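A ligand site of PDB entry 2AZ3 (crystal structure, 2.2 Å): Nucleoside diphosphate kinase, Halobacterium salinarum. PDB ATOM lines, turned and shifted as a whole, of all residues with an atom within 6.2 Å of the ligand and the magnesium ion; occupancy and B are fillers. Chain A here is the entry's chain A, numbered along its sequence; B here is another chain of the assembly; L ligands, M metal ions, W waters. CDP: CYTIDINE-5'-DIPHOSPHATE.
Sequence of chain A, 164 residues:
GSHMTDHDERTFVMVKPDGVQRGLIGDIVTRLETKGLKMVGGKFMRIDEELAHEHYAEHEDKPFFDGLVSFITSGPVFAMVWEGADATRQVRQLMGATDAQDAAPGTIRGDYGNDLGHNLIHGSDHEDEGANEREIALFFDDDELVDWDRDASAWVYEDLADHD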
ATOM      1  N   LYS A  16     -21.627   6.007 -18.053  1.00  0.00           N
ATOM      2  CA  LYS A  16     -20.438   5.281 -17.608  1.00  0.00           C
ATOM      3  C   LYS A  16     -19.201   6.138 -17.795  1.00  0.00           C
ATOM      4  O   LYS A  16     -19.280   7.248 -18.338  1.00  0.00           O
ATOM      5  CB  LYS A  16     -20.348   3.935 -18.292  1.00  0.00           C
ATOM      6  CG  LYS A  16     -21.588   3.036 -18.055  1.00  0.00           C
ATOM      7  CD  LYS A  16     -21.636   1.893 -19.053  1.00  0.00           C
ATOM      8  CE  LYS A  16     -22.598   0.745 -18.675  1.00  0.00           C
ATOM      9  NZ  LYS A  16     -22.188  -0.546 -19.439  1.00  0.00           N
ATOM     10  N   TYR A  56     -22.765  -5.582 -10.279  1.00  0.00           N
ATOM     11  CA  TYR A  56     -22.481  -6.562 -11.323  1.00  0.00           C
ATOM     12  C   TYR A  56     -22.380  -7.997 -10.815  1.00  0.00           C
ATOM     13  O   TYR A  56     -21.782  -8.865 -11.494  1.00  0.00           O
ATOM     14  CB  TYR A  56     -21.177  -6.164 -12.057  1.00  0.00           C
ATOM     15  CG  TYR A  56     -21.326  -4.928 -12.967  1.00  0.00           C
ATOM     16  CD1 TYR A  56     -22.462  -4.783 -13.820  1.00  0.00           C
ATOM     17  CD2 TYR A  56     -20.350  -3.928 -13.036  1.00  0.00           C
ATOM     18  CE1 TYR A  56     -22.619  -3.716 -14.691  1.00  0.00           C
ATOM     19  CE2 TYR A  56     -20.514  -2.801 -13.971  1.00  0.00           C
ATOM     20  CZ  TYR A  56     -21.661  -2.708 -14.767  1.00  0.00           C
ATOM     21  OH  TYR A  56     -21.910  -1.666 -15.667  1.00  0.00           O
ATOM     22  N   GLU A  58     -24.430 -10.482 -10.676  1.00  0.00           N
ATOM     23  CA  GLU A  58     -24.916 -11.451 -11.660  1.00  0.00           C
ATOM     24  C   GLU A  58     -23.933 -11.880 -12.746  1.00  0.00           C
ATOM     25  O   GLU A  58     -24.155 -12.911 -13.375  1.00  0.00           O
ATOM     26  CB  GLU A  58     -26.194 -10.933 -12.351  1.00  0.00           C
ATOM     27  CG  GLU A  58     -25.940  -9.879 -13.432  1.00  0.00           C
ATOM     28  CD  GLU A  58     -27.177  -9.586 -14.306  1.00  0.00           C
ATOM     29  OE1 GLU A  58     -28.087 -10.457 -14.439  1.00  0.00           O
ATOM     30  OE2 GLU A  58     -27.230  -8.451 -14.858  1.00  0.00           O
ATOM     31  N   HIS A  59     -22.873 -11.087 -13.000  1.00  0.00           N
ATOM     32  CA  HIS A  59     -21.888 -11.441 -14.036  1.00  0.00           C
ATOM     33  C   HIS A  59     -20.566 -11.965 -13.436  1.00  0.00           C
ATOM     34  O   HIS A  59     -19.580 -12.158 -14.168  1.00  0.00           O
ATOM     35  CB  HIS A  59     -21.586 -10.248 -14.990  1.00  0.00           C
ATOM     36  CG  HIS A  59     -22.794  -9.635 -15.635  1.00  0.00           C
ATOM     37  ND1 HIS A  59     -23.624 -10.324 -16.493  1.00  0.00           N
ATOM     38  CD2 HIS A  59     -23.322  -8.389 -15.519  1.00  0.00           C
ATOM     39  CE1 HIS A  59     -24.594  -9.521 -16.906  1.00  0.00           C
ATOM     40  NE2 HIS A  59     -24.440  -8.347 -16.328  1.00  0.00           N
ATOM     41  N   PHE A  64     -15.953 -11.535 -18.662  1.00  0.00           N
ATOM     42  CA  PHE A  64     -15.769 -10.120 -18.847  1.00  0.00           C
ATOM     43  C   PHE A  64     -15.912  -9.372 -17.564  1.00  0.00           C
ATOM     44  O   PHE A  64     -15.682  -8.138 -17.536  1.00  0.00           O
ATOM     45  CB  PHE A  64     -16.763  -9.566 -19.873  1.00  0.00           C
ATOM     46  CG  PHE A  64     -18.192  -9.975 -19.638  1.00  0.00           C
ATOM     47  CD1 PHE A  64     -18.979  -9.311 -18.704  1.00  0.00           C
ATOM     48  CD2 PHE A  64     -18.792 -10.991 -20.412  1.00  0.00           C
ATOM     49  CE1 PHE A  64     -20.295  -9.664 -18.515  1.00  0.00           C
ATOM     50  CE2 PHE A  64     -20.132 -11.391 -20.215  1.00  0.00           C
ATOM     51  CZ  PHE A  64     -20.892 -10.707 -19.268  1.00  0.00           C
ATOM     52  N   LEU A  68     -14.934  -5.463 -16.608  1.00  0.00           N
ATOM     53  CA  LEU A  68     -16.110  -4.692 -16.285  1.00  0.00           C
ATOM     54  C   LEU A  68     -15.969  -3.986 -14.974  1.00  0.00           C
ATOM     55  O   LEU A  68     -16.333  -2.831 -14.905  1.00  0.00           O
ATOM     56  CB  LEU A  68     -17.318  -5.607 -16.177  1.00  0.00           C
ATOM     57  CG  LEU A  68     -18.704  -4.970 -16.091  1.00  0.00           C
ATOM     58  CD1 LEU A  68     -19.033  -4.355 -17.390  1.00  0.00           C
ATOM     59  CD2 LEU A  68     -19.720  -6.032 -15.717  1.00  0.00           C
ATOM     60  N   PHE A  71     -13.190  -1.208 -15.561  1.00  0.00           N
ATOM     61  CA  PHE A  71     -13.855  -0.106 -16.305  1.00  0.00           C
ATOM     62  C   PHE A  71     -14.769   0.795 -15.462  1.00  0.00           C
ATOM     63  O   PHE A  71     -14.636   2.019 -15.431  1.00  0.00           O
ATOM     64  CB  PHE A  71     -14.741  -0.642 -17.382  1.00  0.00           C
ATOM     65  CG  PHE A  71     -15.455   0.435 -18.180  1.00  0.00           C
ATOM     66  CD1 PHE A  71     -14.783   1.562 -18.638  1.00  0.00           C
ATOM     67  CD2 PHE A  71     -16.766   0.301 -18.506  1.00  0.00           C
ATOM     68  CE1 PHE A  71     -15.481   2.535 -19.382  1.00  0.00           C
ATOM     69  CE2 PHE A  71     -17.414   1.220 -19.233  1.00  0.00           C
ATOM     70  CZ  PHE A  71     -16.769   2.330 -19.671  1.00  0.00           C
ATOM     71  N   ARG A  92     -34.558   2.050 -21.949  1.00  0.00           N
ATOM     72  CA  ARG A  92     -33.850   1.009 -22.659  1.00  0.00           C
ATOM     73  C   ARG A  92     -33.976   1.235 -24.149  1.00  0.00           C
ATOM     74  O   ARG A  92     -33.083   0.899 -24.865  1.00  0.00           O
ATOM     75  CB  ARG A  92     -34.294  -0.432 -22.279  1.00  0.00           C
ATOM     76  CG  ARG A  92     -33.981  -0.784 -20.817  1.00  0.00           C
ATOM     77  CD  ARG A  92     -32.503  -1.086 -20.549  1.00  0.00           C
ATOM     78  NE  ARG A  92     -32.193  -2.380 -21.084  1.00  0.00           N
ATOM     79  CZ  ARG A  92     -31.248  -3.177 -20.659  1.00  0.00           C
ATOM     80  NH1 ARG A  92     -30.465  -2.834 -19.626  1.00  0.00           N
ATOM     81  NH2 ARG A  92     -31.076  -4.338 -21.285  1.00  0.00           N
ATOM     82  N   MET A  95     -31.645   4.048 -25.365  1.00  0.00           N
ATOM     83  CA  MET A  95     -30.194   3.774 -25.236  1.00  0.00           C
ATOM     84  C   MET A  95     -29.821   2.885 -26.347  1.00  0.00           C
ATOM     85  O   MET A  95     -28.677   2.955 -26.800  1.00  0.00           O
ATOM     86  CB  MET A  95     -29.843   3.013 -23.949  1.00  0.00           C
ATOM     87  CG  MET A  95     -29.723   3.833 -22.726  1.00  0.00           C
ATOM     88  SD  MET A  95     -29.460   2.785 -21.267  1.00  0.00           S
ATOM     89  CE  MET A  95     -30.514   1.551 -21.441  1.00  0.00           C
ATOM     90  N   THR A  98     -27.330  -2.941 -26.198  1.00  0.00           N
ATOM     91  CA  THR A  98     -26.230  -2.988 -25.288  1.00  0.00           C
ATOM     92  C   THR A  98     -24.912  -2.876 -26.024  1.00  0.00           C
ATOM     93  O   THR A  98     -24.090  -2.101 -25.652  1.00  0.00           O
ATOM     94  CB  THR A  98     -26.253  -4.271 -24.528  1.00  0.00           C
ATOM     95  OG1 THR A  98     -27.490  -4.330 -23.820  1.00  0.00           O
ATOM     96  CG2 THR A  98     -25.176  -4.276 -23.420  1.00  0.00           C
ATOM     97  N   ARG A 109     -26.554   4.868 -28.022  1.00  0.00           N
ATOM     98  CA  ARG A 109     -25.352   4.077 -28.347  1.00  0.00           C
ATOM     99  C   ARG A 109     -25.065   4.018 -29.849  1.00  0.00           C
ATOM    100  O   ARG A 109     -23.917   3.957 -30.255  1.00  0.00           O
ATOM    101  CB  ARG A 109     -25.418   2.639 -27.800  1.00  0.00           C
ATOM    102  CG  ARG A 109     -25.200   2.512 -26.319  1.00  0.00           C
ATOM    103  CD  ARG A 109     -25.704   1.268 -25.799  1.00  0.00           C
ATOM    104  NE  ARG A 109     -25.565   1.149 -24.372  1.00  0.00           N
ATOM    105  CZ  ARG A 109     -26.423   0.516 -23.589  1.00  0.00           C
ATOM    106  NH1 ARG A 109     -27.511  -0.082 -24.092  1.00  0.00           N
ATOM    107  NH2 ARG A 109     -26.197   0.488 -22.281  1.00  0.00           N
ATOM    108  N   LEU A 116     -18.786  -2.401 -26.832  1.00  0.00           N
ATOM    109  CA  LEU A 116     -19.690  -3.099 -25.975  1.00  0.00           C
ATOM    110  C   LEU A 116     -19.262  -2.846 -24.543  1.00  0.00           C
ATOM    111  O   LEU A 116     -20.078  -2.633 -23.685  1.00  0.00           O
ATOM    112  CB  LEU A 116     -19.672  -4.598 -26.287  1.00  0.00           C
ATOM    113  CG  LEU A 116     -20.275  -5.484 -25.252  1.00  0.00           C
ATOM    114  CD1 LEU A 116     -21.719  -5.048 -24.944  1.00  0.00           C
ATOM    115  CD2 LEU A 116     -20.242  -6.894 -25.802  1.00  0.00           C
ATOM    116  N   GLY A 117     -17.975  -2.811 -24.266  1.00  0.00           N
ATOM    117  CA  GLY A 117     -17.587  -2.497 -22.901  1.00  0.00           C
ATOM    118  C   GLY A 117     -17.713  -1.030 -22.614  1.00  0.00           C
ATOM    119  O   GLY A 117     -18.226  -0.645 -21.597  1.00  0.00           O
ATOM    120  N   HIS A 118     -17.165  -0.221 -23.503  1.00  0.00           N
ATOM    121  CA  HIS A 118     -17.268   1.250 -23.424  1.00  0.00           C
ATOM    122  C   HIS A 118     -18.544   1.649 -24.166  1.00  0.00           C
ATOM    123  O   HIS A 118     -18.497   2.039 -25.346  1.00  0.00           O
ATOM    124  CB  HIS A 118     -16.026   1.851 -24.039  1.00  0.00           C
ATOM    125  CG  HIS A 118     -14.833   1.773 -23.136  1.00  0.00           C
ATOM    126  ND1 HIS A 118     -14.650   0.734 -22.241  1.00  0.00           N
ATOM    127  CD2 HIS A 118     -13.803   2.608 -22.933  1.00  0.00           C
ATOM    128  CE1 HIS A 118     -13.579   0.955 -21.521  1.00  0.00           C
ATOM    129  NE2 HIS A 118     -13.024   2.070 -21.930  1.00  0.00           N
ATOM    130  N   ASN A 119     -19.705   1.508 -23.508  1.00  0.00           N
ATOM    131  CA  ASN A 119     -21.006   1.740 -24.195  1.00  0.00           C
ATOM    132  C   ASN A 119     -21.895   2.816 -23.547  1.00  0.00           C
ATOM    133  O   ASN A 119     -23.124   2.772 -23.626  1.00  0.00           O
ATOM    134  CB  ASN A 119     -21.769   0.409 -24.396  1.00  0.00           C
ATOM    135  CG  ASN A 119     -22.281  -0.226 -23.069  1.00  0.00           C
ATOM    136  OD1 ASN A 119     -21.879   0.210 -21.993  1.00  0.00           O
ATOM    137  ND2 ASN A 119     -23.107  -1.289 -23.159  1.00  0.00           N
ATOM    138  N   ILE A 121     -23.515   4.269 -21.235  1.00  0.00           N
ATOM    139  CA  ILE A 121     -24.534   4.405 -20.238  1.00  0.00           C
ATOM    140  C   ILE A 121     -25.143   3.078 -19.811  1.00  0.00           C
ATOM    141  O   ILE A 121     -25.049   2.025 -20.506  1.00  0.00           O
ATOM    142  CB  ILE A 121     -25.572   5.519 -20.723  1.00  0.00           C
ATOM    143  CG1 ILE A 121     -27.006   5.208 -20.483  1.00  0.00           C
ATOM    144  CG2 ILE A 121     -25.438   5.786 -22.179  1.00  0.00           C
ATOM    145  CD1 ILE A 121     -27.934   6.356 -20.855  1.00  0.00           C
ATOM    146  N   HIS A 122     -25.737   3.092 -18.646  1.00  0.00           N
ATOM    147  CA  HIS A 122     -26.481   1.904 -18.190  1.00  0.00           C
ATOM    148  C   HIS A 122     -27.862   2.344 -17.801  1.00  0.00           C
ATOM    149  O   HIS A 122     -28.085   3.409 -17.300  1.00  0.00           O
ATOM    150  CB  HIS A 122     -25.807   1.229 -16.980  1.00  0.00           C
ATOM    151  CG  HIS A 122     -26.721   0.300 -16.240  1.00  0.00           C
ATOM    152  ND1 HIS A 122     -26.726  -1.060 -16.455  1.00  0.00           N
ATOM    153  CD2 HIS A 122     -27.741   0.544 -15.389  1.00  0.00           C
ATOM    154  CE1 HIS A 122     -27.661  -1.622 -15.721  1.00  0.00           C
ATOM    155  NE2 HIS A 122     -28.317  -0.682 -15.082  1.00  0.00           N
ATOM    156  N   GLY A 123     -28.831   1.498 -18.055  1.00  0.00           N
ATOM    157  CA  GLY A 123     -30.160   1.801 -17.567  1.00  0.00           C
ATOM    158  C   GLY A 123     -30.743   0.499 -17.149  1.00  0.00           C
ATOM    159  O   GLY A 123     -30.377  -0.496 -17.759  1.00  0.00           O
ATOM    160  N   SER A 124     -31.673   0.506 -16.200  1.00  0.00           N
ATOM    161  CA  SER A 124     -32.135  -0.780 -15.656  1.00  0.00           C
ATOM    162  C   SER A 124     -32.863  -1.512 -16.735  1.00  0.00           C
ATOM    163  O   SER A 124     -33.462  -0.886 -17.592  1.00  0.00           O
ATOM    164  CB  SER A 124     -33.064  -0.641 -14.470  1.00  0.00           C
ATOM    165  OG  SER A 124     -32.615   0.349 -13.575  1.00  0.00           O
ATOM    166  N   ASP A 125     -32.780  -2.835 -16.715  1.00  0.00           N
ATOM    167  CA  ASP A 125     -33.437  -3.725 -17.678  1.00  0.00           C
ATOM    168  C   ASP A 125     -34.862  -3.942 -17.233  1.00  0.00           C
ATOM    169  O   ASP A 125     -35.093  -4.515 -16.206  1.00  0.00           O
ATOM    170  CB  ASP A 125     -32.618  -5.036 -17.720  1.00  0.00           C
ATOM    171  CG  ASP A 125     -33.058  -6.002 -18.793  1.00  0.00           C
ATOM    172  OD1 ASP A 125     -33.984  -5.697 -19.678  1.00  0.00           O
ATOM    173  OD2 ASP A 125     -32.531  -7.158 -18.773  1.00  0.00           O
ATOM    174  N   ASP A 128     -35.828  -7.612 -16.506  1.00  0.00           N
ATOM    175  CA  ASP A 128     -35.524  -8.215 -15.217  1.00  0.00           C
ATOM    176  C   ASP A 128     -36.350  -7.571 -14.084  1.00  0.00           C
ATOM    177  O   ASP A 128     -36.080  -6.440 -13.645  1.00  0.00           O
ATOM    178  CB  ASP A 128     -34.041  -8.127 -14.909  1.00  0.00           C
ATOM    179  CG  ASP A 128     -33.666  -9.060 -13.819  1.00  0.00           C
ATOM    180  OD1 ASP A 128     -33.490 -10.275 -14.100  1.00  0.00           O
ATOM    181  OD2 ASP A 128     -33.587  -8.692 -12.644  1.00  0.00           O
ATOM    182  N   GLU B 158     -12.360  -0.489 -25.366  1.00  0.00           N
ATOM    183  CA  GLU B 158     -11.671  -1.182 -24.248  1.00  0.00           C
ATOM    184  C   GLU B 158     -10.196  -1.459 -24.544  1.00  0.00           C
ATOM    185  O   GLU B 158      -9.881  -1.949 -25.651  1.00  0.00           O
ATOM    186  CB  GLU B 158     -12.324  -2.509 -23.948  1.00  0.00           C
ATOM    187  CG  GLU B 158     -13.582  -2.443 -23.132  1.00  0.00           C
ATOM    188  CD  GLU B 158     -14.155  -3.836 -22.814  1.00  0.00           C
ATOM    189  OE1 GLU B 158     -14.455  -4.667 -23.734  1.00  0.00           O
ATOM    190  OE2 GLU B 158     -14.316  -4.093 -21.607  1.00  0.00           O
HETATM  191  O3B CDP L   1     -26.463  -2.869 -19.290  1.00  0.00           O
HETATM  192  PB  CDP L   1     -27.295  -4.178 -19.736  1.00  0.00           P
HETATM  193  O1B CDP L   1     -28.329  -4.583 -18.566  1.00  0.00           O
HETATM  194  O2B CDP L   1     -28.131  -3.937 -21.076  1.00  0.00           O
HETATM  195  O3A CDP L   1     -26.316  -5.336 -20.200  1.00  0.00           O
HETATM  196  PA  CDP L   1     -25.799  -6.633 -19.412  1.00  0.00           P
HETATM  197  O1A CDP L   1     -26.381  -6.834 -17.921  1.00  0.00           O
HETATM  198  O2A CDP L   1     -26.157  -7.762 -20.463  1.00  0.00           O
HETATM  199  O5' CDP L   1     -24.243  -6.410 -19.347  1.00  0.00           O
HETATM  200  C5' CDP L   1     -23.850  -5.356 -18.505  1.00  0.00           C
HETATM  201  C4' CDP L   1     -22.702  -4.597 -19.147  1.00  0.00           C
HETATM  202  O4' CDP L   1     -21.463  -5.292 -19.125  1.00  0.00           O
HETATM  203  C3' CDP L   1     -22.944  -4.110 -20.549  1.00  0.00           C
HETATM  204  O3' CDP L   1     -23.409  -2.786 -20.598  1.00  0.00           O
HETATM  205  C2' CDP L   1     -21.644  -4.315 -21.239  1.00  0.00           C
HETATM  206  O2' CDP L   1     -21.007  -3.056 -21.246  1.00  0.00           O
HETATM  207  C1' CDP L   1     -20.758  -5.150 -20.342  1.00  0.00           C
HETATM  208  N1  CDP L   1     -20.431  -6.382 -21.093  1.00  0.00           N
HETATM  209  C2  CDP L   1     -19.081  -6.488 -21.472  1.00  0.00           C
HETATM  210  O2  CDP L   1     -18.298  -5.600 -21.108  1.00  0.00           O
HETATM  211  N3  CDP L   1     -18.588  -7.509 -22.172  1.00  0.00           N
HETATM  212  C4  CDP L   1     -19.434  -8.466 -22.568  1.00  0.00           C
HETATM  213  N4  CDP L   1     -18.854  -9.451 -23.273  1.00  0.00           N
HETATM  214  C5  CDP L   1     -20.794  -8.408 -22.250  1.00  0.00           C
HETATM  215  C6  CDP L   1     -21.301  -7.318 -21.496  1.00  0.00           C
HETATM  216 MG    MG M   1     -28.379  -7.822 -16.779  1.00  0.00          MG
HETATM  217  O   HOH W   1     -19.309  -1.366 -19.036  1.00  0.00           O
HETATM  218  O   HOH W   2     -28.034  -0.801 -20.008  1.00  0.00           O
HETATM  219  O   HOH W   3     -24.556  -1.741 -17.781  1.00  0.00           O
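O of Leu 116 lies within hydrogen-bond range of O2' of the ligand (2.6 Å). NZ of Lys 16 is in hydrogen-bond range of O3' of the ligand. OG1 of Thr 98 sits at hydrogen-bond distance from O2B of the ligand, 2.8 Å away. A ring nitrogen (NE2) of His 59 lies close to an oxygen (O1A) of the ligand (2.9 Å). NH1 of Arg 92 is in salt-bridge range of O1B of the ligand (3.0 Å). ND2 of Asn 119 sits at hydrogen-bond distance from O3' of the ligand (3.0 Å). ND1 of His 122 is in hydrogen-bond range of O3B of the ligand (3.4 Å).
The side-chain carboxylate (OE2) of Glu 58 lies close to a ring nitrogen (NE2) of His 59 (3.2 Å). The backbone carbonyl oxygen (O) of Leu 116 sits close to the side-chain amide nitrogen (ND2) of Asn 119 (3.4 Å). The side-chain amide oxygen (OD1) of Asn 119 lies within hydrogen-bond range of the side-chain amino group (NZ) of Lys 16, at 2.7 Å. O of Thr 98 is in hydrogen-bond range of ND2 of Asn 119 (2.8 Å). The guanidinium group of Arg 92 lies within salt-bridge range of the side-chain carboxylate of Asp 125 (3.6 Å). NH1 of Arg 92 sits at hydrogen-bond distance from O of Gly 123 (3.0 Å). O of Asn 119 is in hydrogen-bond range of NE of Arg 109 (3.0 Å).
Merely in contact with the ligand: Leu 68 (3.1 Å), Phe 64 (3.2 Å) and Gly 117 (3.7 Å). Hydrophobic or aromatic side chains within 4 Å of the ligand: His 59, Phe 64, Leu 68, Leu 116 and His 122. Within 4 Å of the ligand: Lys 16, Glu 58, His 59, Phe 64, Leu 68, Arg 92, Thr 98, Leu 116, Gly 117, Asn 119 and His 122. The nearest printed residue that does not touch the ligand is Glu 158 of chain B (4.3 Å).
Merely in contact with the magnesium ion: His 59. Along chain A the residues within 4 Å of the magnesium ion span positions 58 to 59. The nearest printed residue that does not touch the magnesium ion is Asp 125 (4.7 Å).
The magnesium ion is bound by the side-chain carboxylate of Glu 58 and an oxygen (O1A) of the ligand.
Water W3 lies within hydrogen-bond range of ND1 of His 122 (2.6 Å), O3B of the ligand (2.7 Å), NZ of Lys 16 (3.1 Å) and OH of Tyr 56 (3.4 Å). Water W1 lies within hydrogen-bond range of O of Gly 117, NZ of Lys 16 and O2' of the ligand.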
